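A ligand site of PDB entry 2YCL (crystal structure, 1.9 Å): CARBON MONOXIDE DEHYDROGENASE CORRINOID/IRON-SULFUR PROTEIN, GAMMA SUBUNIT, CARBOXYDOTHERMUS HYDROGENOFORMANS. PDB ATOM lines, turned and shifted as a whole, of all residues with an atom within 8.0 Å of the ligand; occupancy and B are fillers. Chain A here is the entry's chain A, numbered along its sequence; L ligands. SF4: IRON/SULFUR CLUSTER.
The backbone NH (N) of Lys 15 sits close to a sulfur (S1) of the ligand, 3.7 Å away.
An iron atom (FE3) of the ligand is bound by the side-chain sulfur (SG) of Cys 17 (2.7 Å).
A sulfur (S4) of the ligand sits close to the backbone NH (N) of Lys 18 (3.3 Å).
An iron atom (FE1) of the ligand is bound by the side-chain sulfur of Cys 20, at 2.5 Å.
The backbone NH (N) of Cys 17 lies close to a sulfur (S4) of the ligand (3.4 Å).
N of Cys 20 sits close to S2 of the ligand, 3.5 Å away.
An iron atom (FE2) of the ligand is bound by the side-chain sulfur (SG) of Cys 25 (2.4 Å).
The side-chain sulfur of Cys 42 binds an iron atom (FE4) of the ligand (2.3 Å).
The side-chain sulfur (SG) of Cys 20 sits close to the backbone NH (N) of Gln 22.
N of Lys 14 lies close to SG of Cys 25.
The side-chain amide oxygen (OD1) of Asn 16 lies within hydrogen-bond range of the backbone NH (N) of Cys 25, 3.0 Å away.
The backbone NH of Glu 19 lies close to the side-chain sulfur of Cys 17.
N of Tyr 44 sits close to SG of Cys 42, at 3.6 Å.
The side-chain amino group (NZ) of Lys 18 lies within hydrogen-bond range of the backbone carbonyl oxygen (O) of Pro 23 (3.1 Å).
SG of Cys 42 lies close to N of Val 45, at 3.3 Å.
The side-chain sulfur (SG) of Cys 25 sits close to the backbone NH (N) of Lys 15.
CB of Pro 13 touches S1 of the ligand (3.7 Å).
Asn 16 touches the ligand.
CD2 of Phe 28 touches S3 of the ligand, at 3.4 Å.
CD of Pro 43 touches S2 of the ligand, 3.8 Å away.
Of the 28 residues printed, 10 come within 4 Å of the ligand.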
ATOM      1  N   ILE A   8      14.091 -19.542   2.162  1.00  0.00           N
ATOM      2  CA  ILE A   8      15.230 -19.004   1.439  1.00  0.00           C
ATOM      3  C   ILE A   8      14.817 -17.844   0.537  1.00  0.00           C
ATOM      4  O   ILE A   8      15.673 -17.090   0.071  1.00  0.00           O
ATOM      5  CB  ILE A   8      15.954 -20.113   0.621  1.00  0.00           C
ATOM      6  CG1 ILE A   8      15.356 -20.218  -0.781  1.00  0.00           C
ATOM      7  CG2 ILE A   8      15.900 -21.459   1.348  1.00  0.00           C
ATOM      8  CD1 ILE A   8      16.141 -19.431  -1.822  1.00  0.00           C
ATOM      9  N   TYR A   9      13.521 -17.680   0.302  1.00  0.00           N
ATOM     10  CA  TYR A   9      13.031 -16.561  -0.514  1.00  0.00           C
ATOM     11  C   TYR A   9      13.050 -15.213   0.204  1.00  0.00           C
ATOM     12  O   TYR A   9      13.211 -14.175  -0.426  1.00  0.00           O
ATOM     13  CB  TYR A   9      11.596 -16.791  -1.001  1.00  0.00           C
ATOM     14  CG  TYR A   9      10.900 -15.480  -1.371  1.00  0.00           C
ATOM     15  CD1 TYR A   9      10.230 -14.733  -0.400  1.00  0.00           C
ATOM     16  CD2 TYR A   9      10.956 -14.970  -2.659  1.00  0.00           C
ATOM     17  CE1 TYR A   9       9.607 -13.536  -0.720  1.00  0.00           C
ATOM     18  CE2 TYR A   9      10.333 -13.774  -2.979  1.00  0.00           C
ATOM     19  CZ  TYR A   9       9.665 -13.059  -2.012  1.00  0.00           C
ATOM     20  OH  TYR A   9       9.046 -11.864  -2.318  1.00  0.00           O
ATOM     21  N   LEU A  12      15.928 -12.996  -0.786  1.00  0.00           N
ATOM     22  CA  LEU A  12      16.229 -12.813  -2.212  1.00  0.00           C
ATOM     23  C   LEU A  12      15.999 -11.390  -2.708  1.00  0.00           C
ATOM     24  O   LEU A  12      15.296 -10.618  -2.066  1.00  0.00           O
ATOM     25  CB  LEU A  12      15.398 -13.788  -3.044  1.00  0.00           C
ATOM     26  CG  LEU A  12      15.785 -15.251  -2.893  1.00  0.00           C
ATOM     27  CD1 LEU A  12      14.866 -16.159  -3.715  1.00  0.00           C
ATOM     28  CD2 LEU A  12      17.225 -15.449  -3.294  1.00  0.00           C
ATOM     29  N   PRO A  13      16.596 -11.049  -3.866  1.00  0.00           N
ATOM     30  CA  PRO A  13      16.470  -9.714  -4.475  1.00  0.00           C
ATOM     31  C   PRO A  13      15.040  -9.328  -4.836  1.00  0.00           C
ATOM     32  O   PRO A  13      14.737  -8.133  -4.910  1.00  0.00           O
ATOM     33  CB  PRO A  13      17.340  -9.817  -5.730  1.00  0.00           C
ATOM     34  CG  PRO A  13      18.333 -10.870  -5.409  1.00  0.00           C
ATOM     35  CD  PRO A  13      17.608 -11.870  -4.552  1.00  0.00           C
ATOM     36  N   LYS A  14      14.169 -10.312  -5.051  1.00  0.00           N
ATOM     37  CA  LYS A  14      12.752 -10.068  -5.317  1.00  0.00           C
ATOM     38  C   LYS A  14      12.481  -9.342  -6.631  1.00  0.00           C
ATOM     39  O   LYS A  14      11.458  -8.681  -6.777  1.00  0.00           O
ATOM     40  CB  LYS A  14      12.118  -9.244  -4.188  1.00  0.00           C
ATOM     41  CG  LYS A  14      12.325  -9.824  -2.813  1.00  0.00           C
ATOM     42  CD  LYS A  14      11.626  -8.976  -1.765  1.00  0.00           C
ATOM     43  CE  LYS A  14      12.184  -9.244  -0.392  1.00  0.00           C
ATOM     44  NZ  LYS A  14      12.295 -10.701  -0.115  1.00  0.00           N
ATOM     45  N   LYS A  15      13.390  -9.474  -7.589  1.00  0.00           N
ATOM     46  CA  LYS A  15      13.243  -8.797  -8.877  1.00  0.00           C
ATOM     47  C   LYS A  15      12.319  -9.545  -9.840  1.00  0.00           C
ATOM     48  O   LYS A  15      11.795  -8.956 -10.781  1.00  0.00           O
ATOM     49  CB  LYS A  15      14.605  -8.605  -9.540  1.00  0.00           C
ATOM     50  CG  LYS A  15      15.572  -7.770  -8.723  1.00  0.00           C
ATOM     51  CD  LYS A  15      17.004  -8.061  -9.131  1.00  0.00           C
ATOM     52  CE  LYS A  15      17.274  -7.728 -10.593  1.00  0.00           C
ATOM     53  NZ  LYS A  15      17.232  -6.266 -10.883  1.00  0.00           N
ATOM     54  N   ASN A  16      12.134 -10.842  -9.595  1.00  0.00           N
ATOM     55  CA  ASN A  16      11.411 -11.713 -10.524  1.00  0.00           C
ATOM     56  C   ASN A  16      11.889 -11.483 -11.953  1.00  0.00           C
ATOM     57  O   ASN A  16      11.082 -11.425 -12.879  1.00  0.00           O
ATOM     58  CB  ASN A  16       9.892 -11.483 -10.451  1.00  0.00           C
ATOM     59  CG  ASN A  16       9.324 -11.722  -9.063  1.00  0.00           C
ATOM     60  OD1 ASN A  16       9.304 -12.852  -8.572  1.00  0.00           O
ATOM     61  ND2 ASN A  16       8.826 -10.666  -8.441  1.00  0.00           N
ATOM     62  N   CYS A  17      13.197 -11.341 -12.131  1.00  0.00           N
ATOM     63  CA  CYS A  17      13.753 -11.030 -13.450  1.00  0.00           C
ATOM     64  C   CYS A  17      14.058 -12.285 -14.269  1.00  0.00           C
ATOM     65  O   CYS A  17      14.498 -12.203 -15.411  1.00  0.00           O
ATOM     66  CB  CYS A  17      15.023 -10.186 -13.305  1.00  0.00           C
ATOM     67  SG  CYS A  17      16.421 -11.087 -12.595  1.00  0.00           S
ATOM     68  N   LYS A  18      13.826 -13.456 -13.667  1.00  0.00           N
ATOM     69  CA  LYS A  18      13.910 -14.727 -14.386  1.00  0.00           C
ATOM     70  C   LYS A  18      15.326 -15.142 -14.808  1.00  0.00           C
ATOM     71  O   LYS A  18      15.510 -16.222 -15.362  1.00  0.00           O
ATOM     72  CB  LYS A  18      13.001 -14.693 -15.618  1.00  0.00           C
ATOM     73  CG  LYS A  18      11.524 -14.473 -15.307  1.00  0.00           C
ATOM     74  CD  LYS A  18      10.714 -14.328 -16.595  1.00  0.00           C
ATOM     75  CE  LYS A  18       9.235 -14.141 -16.323  1.00  0.00           C
ATOM     76  NZ  LYS A  18       8.587 -15.387 -15.828  1.00  0.00           N
ATOM     77  N   GLU A  19      16.317 -14.290 -14.550  1.00  0.00           N
ATOM     78  CA  GLU A  19      17.689 -14.527 -15.010  1.00  0.00           C
ATOM     79  C   GLU A  19      18.336 -15.790 -14.437  1.00  0.00           C
ATOM     80  O   GLU A  19      19.390 -16.213 -14.908  1.00  0.00           O
ATOM     81  CB  GLU A  19      18.570 -13.317 -14.682  1.00  0.00           C
ATOM     82  CG  GLU A  19      18.308 -12.097 -15.535  1.00  0.00           C
ATOM     83  CD  GLU A  19      19.190 -10.940 -15.138  1.00  0.00           C
ATOM     84  OE1 GLU A  19      20.217 -11.178 -14.483  1.00  0.00           O
ATOM     85  OE2 GLU A  19      18.851  -9.781 -15.470  1.00  0.00           O
ATOM     86  N   CYS A  20      17.722 -16.367 -13.427  1.00  0.00           N
ATOM     87  CA  CYS A  20      18.233 -17.596 -12.826  1.00  0.00           C
ATOM     88  C   CYS A  20      17.648 -18.806 -13.543  1.00  0.00           C
ATOM     89  O   CYS A  20      17.891 -19.947 -13.159  1.00  0.00           O
ATOM     90  CB  CYS A  20      17.828 -17.650 -11.366  1.00  0.00           C
ATOM     91  SG  CYS A  20      16.044 -17.559 -11.154  1.00  0.00           S
ATOM     92  N   GLY A  21      16.848 -18.529 -14.572  1.00  0.00           N
ATOM     93  CA  GLY A  21      16.154 -19.567 -15.301  1.00  0.00           C
ATOM     94  C   GLY A  21      14.718 -19.757 -14.846  1.00  0.00           C
ATOM     95  O   GLY A  21      13.895 -20.259 -15.609  1.00  0.00           O
ATOM     96  N   GLN A  22      14.411 -19.350 -13.611  1.00  0.00           N
ATOM     97  CA  GLN A  22      13.075 -19.534 -13.051  1.00  0.00           C
ATOM     98  C   GLN A  22      12.138 -18.363 -13.348  1.00  0.00           C
ATOM     99  O   GLN A  22      12.593 -17.248 -13.591  1.00  0.00           O
ATOM    100  CB  GLN A  22      13.139 -19.785 -11.547  1.00  0.00           C
ATOM    101  CG  GLN A  22      13.675 -21.150 -11.186  1.00  0.00           C
ATOM    102  CD  GLN A  22      13.312 -22.188 -12.220  1.00  0.00           C
ATOM    103  OE1 GLN A  22      14.011 -22.367 -13.224  1.00  0.00           O
ATOM    104  NE2 GLN A  22      12.189 -22.865 -12.002  1.00  0.00           N
ATOM    105  N   PRO A  23      10.829 -18.628 -13.335  1.00  0.00           N
ATOM    106  CA  PRO A  23       9.808 -17.594 -13.597  1.00  0.00           C
ATOM    107  C   PRO A  23       9.707 -16.509 -12.505  1.00  0.00           C
ATOM    108  O   PRO A  23       9.441 -15.347 -12.836  1.00  0.00           O
ATOM    109  CB  PRO A  23       8.515 -18.396 -13.695  1.00  0.00           C
ATOM    110  CG  PRO A  23       8.781 -19.674 -12.952  1.00  0.00           C
ATOM    111  CD  PRO A  23      10.234 -19.957 -13.158  1.00  0.00           C
ATOM    112  N   THR A  24       9.898 -16.882 -11.240  1.00  0.00           N
ATOM    113  CA  THR A  24       9.806 -15.919 -10.139  1.00  0.00           C
ATOM    114  C   THR A  24      10.778 -16.250  -9.003  1.00  0.00           C
ATOM    115  O   THR A  24      11.193 -17.390  -8.854  1.00  0.00           O
ATOM    116  CB  THR A  24       8.383 -15.894  -9.520  1.00  0.00           C
ATOM    117  OG1 THR A  24       8.153 -17.127  -8.813  1.00  0.00           O
ATOM    118  CG2 THR A  24       7.319 -15.718 -10.598  1.00  0.00           C
ATOM    119  N   CYS A  25      11.122 -15.244  -8.210  1.00  0.00           N
ATOM    120  CA  CYS A  25      11.978 -15.453  -7.045  1.00  0.00           C
ATOM    121  C   CYS A  25      11.496 -16.603  -6.183  1.00  0.00           C
ATOM    122  O   CYS A  25      12.282 -17.441  -5.739  1.00  0.00           O
ATOM    123  CB  CYS A  25      12.007 -14.190  -6.189  1.00  0.00           C
ATOM    124  SG  CYS A  25      12.941 -12.872  -6.925  1.00  0.00           S
ATOM    125  N   LEU A  26      10.191 -16.647  -5.923  1.00  0.00           N
ATOM    126  CA  LEU A  26       9.618 -17.653  -5.059  1.00  0.00           C
ATOM    127  C   LEU A  26       9.820 -19.043  -5.660  1.00  0.00           C
ATOM    128  O   LEU A  26      10.076 -20.007  -4.946  1.00  0.00           O
ATOM    129  CB  LEU A  26       8.136 -17.368  -4.822  1.00  0.00           C
ATOM    130  CG  LEU A  26       7.372 -18.329  -3.912  1.00  0.00           C
ATOM    131  CD1 LEU A  26       7.908 -18.296  -2.492  1.00  0.00           C
ATOM    132  CD2 LEU A  26       5.876 -18.015  -3.950  1.00  0.00           C
ATOM    133  N   ALA A  27       9.730 -19.133  -6.987  1.00  0.00           N
ATOM    134  CA  ALA A  27       9.919 -20.381  -7.705  1.00  0.00           C
ATOM    135  C   ALA A  27      11.396 -20.717  -7.945  1.00  0.00           C
ATOM    136  O   ALA A  27      11.734 -21.852  -8.276  1.00  0.00           O
ATOM    137  CB  ALA A  27       9.175 -20.339  -9.029  1.00  0.00           C
ATOM    138  N   PHE A  28      12.283 -19.731  -7.779  1.00  0.00           N
ATOM    139  CA  PHE A  28      13.713 -20.000  -7.830  1.00  0.00           C
ATOM    140  C   PHE A  28      14.097 -20.685  -6.538  1.00  0.00           C
ATOM    141  O   PHE A  28      14.798 -21.696  -6.528  1.00  0.00           O
ATOM    142  CB  PHE A  28      14.519 -18.710  -7.998  1.00  0.00           C
ATOM    143  CG  PHE A  28      16.000 -18.906  -7.790  1.00  0.00           C
ATOM    144  CD1 PHE A  28      16.767 -19.563  -8.745  1.00  0.00           C
ATOM    145  CD2 PHE A  28      16.623 -18.441  -6.639  1.00  0.00           C
ATOM    146  CE1 PHE A  28      18.129 -19.733  -8.567  1.00  0.00           C
ATOM    147  CE2 PHE A  28      17.980 -18.610  -6.452  1.00  0.00           C
ATOM    148  CZ  PHE A  28      18.744 -19.254  -7.412  1.00  0.00           C
ATOM    149  N   ALA A  29      13.614 -20.115  -5.437  1.00  0.00           N
ATOM    150  CA  ALA A  29      13.861 -20.670  -4.116  1.00  0.00           C
ATOM    151  C   ALA A  29      13.395 -22.119  -4.054  1.00  0.00           C
ATOM    152  O   ALA A  29      14.060 -22.958  -3.441  1.00  0.00           O
ATOM    153  CB  ALA A  29      13.154 -19.830  -3.082  1.00  0.00           C
ATOM    154  N   ILE A  32      15.910 -24.440  -5.739  1.00  0.00           N
ATOM    155  CA  ILE A  32      17.089 -24.745  -4.905  1.00  0.00           C
ATOM    156  C   ILE A  32      16.735 -25.634  -3.711  1.00  0.00           C
ATOM    157  O   ILE A  32      17.556 -26.432  -3.259  1.00  0.00           O
ATOM    158  CB  ILE A  32      17.808 -23.465  -4.376  1.00  0.00           C
ATOM    159  CG1 ILE A  32      17.118 -22.906  -3.135  1.00  0.00           C
ATOM    160  CG2 ILE A  32      17.924 -22.402  -5.464  1.00  0.00           C
ATOM    161  CD1 ILE A  32      17.989 -21.990  -2.327  1.00  0.00           C
ATOM    162  N   GLY A  38      21.348 -23.773  -7.576  1.00  0.00           N
ATOM    163  CA  GLY A  38      22.122 -23.177  -6.494  1.00  0.00           C
ATOM    164  C   GLY A  38      21.939 -21.669  -6.398  1.00  0.00           C
ATOM    165  O   GLY A  38      21.449 -21.028  -7.323  1.00  0.00           O
ATOM    166  N   LEU A  39      22.406 -21.090  -5.280  1.00  0.00           N
ATOM    167  CA  LEU A  39      22.265 -19.659  -5.032  1.00  0.00           C
ATOM    168  C   LEU A  39      23.020 -18.849  -6.071  1.00  0.00           C
ATOM    169  O   LEU A  39      22.646 -17.731  -6.411  1.00  0.00           O
ATOM    170  CB  LEU A  39      22.775 -19.293  -3.642  1.00  0.00           C
ATOM    171  CG  LEU A  39      21.825 -19.613  -2.489  1.00  0.00           C
ATOM    172  CD1 LEU A  39      21.609 -21.107  -2.386  1.00  0.00           C
ATOM    173  CD2 LEU A  39      22.339 -19.036  -1.178  1.00  0.00           C
ATOM    174  N   ALA A  41      23.039 -19.151  -9.089  1.00  0.00           N
ATOM    175  CA  ALA A  41      22.233 -18.941 -10.299  1.00  0.00           C
ATOM    176  C   ALA A  41      21.550 -17.571 -10.313  1.00  0.00           C
ATOM    177  O   ALA A  41      21.227 -17.043 -11.370  1.00  0.00           O
ATOM    178  CB  ALA A  41      21.190 -20.038 -10.436  1.00  0.00           C
ATOM    179  N   CYS A  42      21.315 -17.012  -9.123  1.00  0.00           N
ATOM    180  CA  CYS A  42      20.794 -15.660  -9.008  1.00  0.00           C
ATOM    181  C   CYS A  42      21.956 -14.676  -8.879  1.00  0.00           C
ATOM    182  O   CYS A  42      22.663 -14.691  -7.874  1.00  0.00           O
ATOM    183  CB  CYS A  42      19.878 -15.539  -7.791  1.00  0.00           C
ATOM    184  SG  CYS A  42      19.500 -13.804  -7.352  1.00  0.00           S
ATOM    185  N   PRO A  43      22.146 -13.834  -9.904  1.00  0.00           N
ATOM    186  CA  PRO A  43      23.275 -12.895  -9.916  1.00  0.00           C
ATOM    187  C   PRO A  43      23.156 -11.752  -8.902  1.00  0.00           C
ATOM    188  O   PRO A  43      24.173 -11.176  -8.514  1.00  0.00           O
ATOM    189  CB  PRO A  43      23.267 -12.353 -11.345  1.00  0.00           C
ATOM    190  CG  PRO A  43      21.857 -12.505 -11.803  1.00  0.00           C
ATOM    191  CD  PRO A  43      21.298 -13.716 -11.102  1.00  0.00           C
ATOM    192  N   TYR A  44      21.927 -11.413  -8.520  1.00  0.00           N
ATOM    193  CA  TYR A  44      21.683 -10.246  -7.674  1.00  0.00           C
ATOM    194  C   TYR A  44      21.605 -10.504  -6.158  1.00  0.00           C
ATOM    195  O   TYR A  44      21.562  -9.549  -5.383  1.00  0.00           O
ATOM    196  CB  TYR A  44      20.410  -9.561  -8.174  1.00  0.00           C
ATOM    197  CG  TYR A  44      20.457  -9.344  -9.662  1.00  0.00           C
ATOM    198  CD1 TYR A  44      21.269  -8.370 -10.222  1.00  0.00           C
ATOM    199  CD2 TYR A  44      19.692 -10.141 -10.513  1.00  0.00           C
ATOM    200  CE1 TYR A  44      21.323  -8.184 -11.575  1.00  0.00           C
ATOM    201  CE2 TYR A  44      19.735  -9.951 -11.884  1.00  0.00           C
ATOM    202  CZ  TYR A  44      20.554  -8.968 -12.408  1.00  0.00           C
ATOM    203  OH  TYR A  44      20.608  -8.772 -13.775  1.00  0.00           O
ATOM    204  N   VAL A  45      21.587 -11.766  -5.738  1.00  0.00           N
ATOM    205  CA  VAL A  45      21.487 -12.061  -4.315  1.00  0.00           C
ATOM    206  C   VAL A  45      22.656 -11.427  -3.559  1.00  0.00           C
ATOM    207  O   VAL A  45      23.809 -11.627  -3.907  1.00  0.00           O
ATOM    208  CB  VAL A  45      21.438 -13.583  -4.033  1.00  0.00           C
ATOM    209  CG1 VAL A  45      22.657 -14.290  -4.622  1.00  0.00           C
ATOM    210  CG2 VAL A  45      21.328 -13.850  -2.531  1.00  0.00           C
HETATM  211 FE1  SF4 L   1      15.812 -15.364  -9.964  1.00  0.00          FE
HETATM  212 FE2  SF4 L   1      14.795 -13.545  -8.369  1.00  0.00          FE
HETATM  213 FE3  SF4 L   1      15.869 -12.920 -10.663  1.00  0.00          FE
HETATM  214 FE4  SF4 L   1      17.561 -13.584  -8.525  1.00  0.00          FE
HETATM  215  S1  SF4 L   1      16.127 -11.714  -8.652  1.00  0.00           S
HETATM  216  S2  SF4 L   1      17.584 -14.237 -10.636  1.00  0.00           S
HETATM  217  S3  SF4 L   1      16.130 -15.194  -7.602  1.00  0.00           S
HETATM  218  S4  SF4 L   1      14.068 -14.169 -10.488  1.00  0.00           S
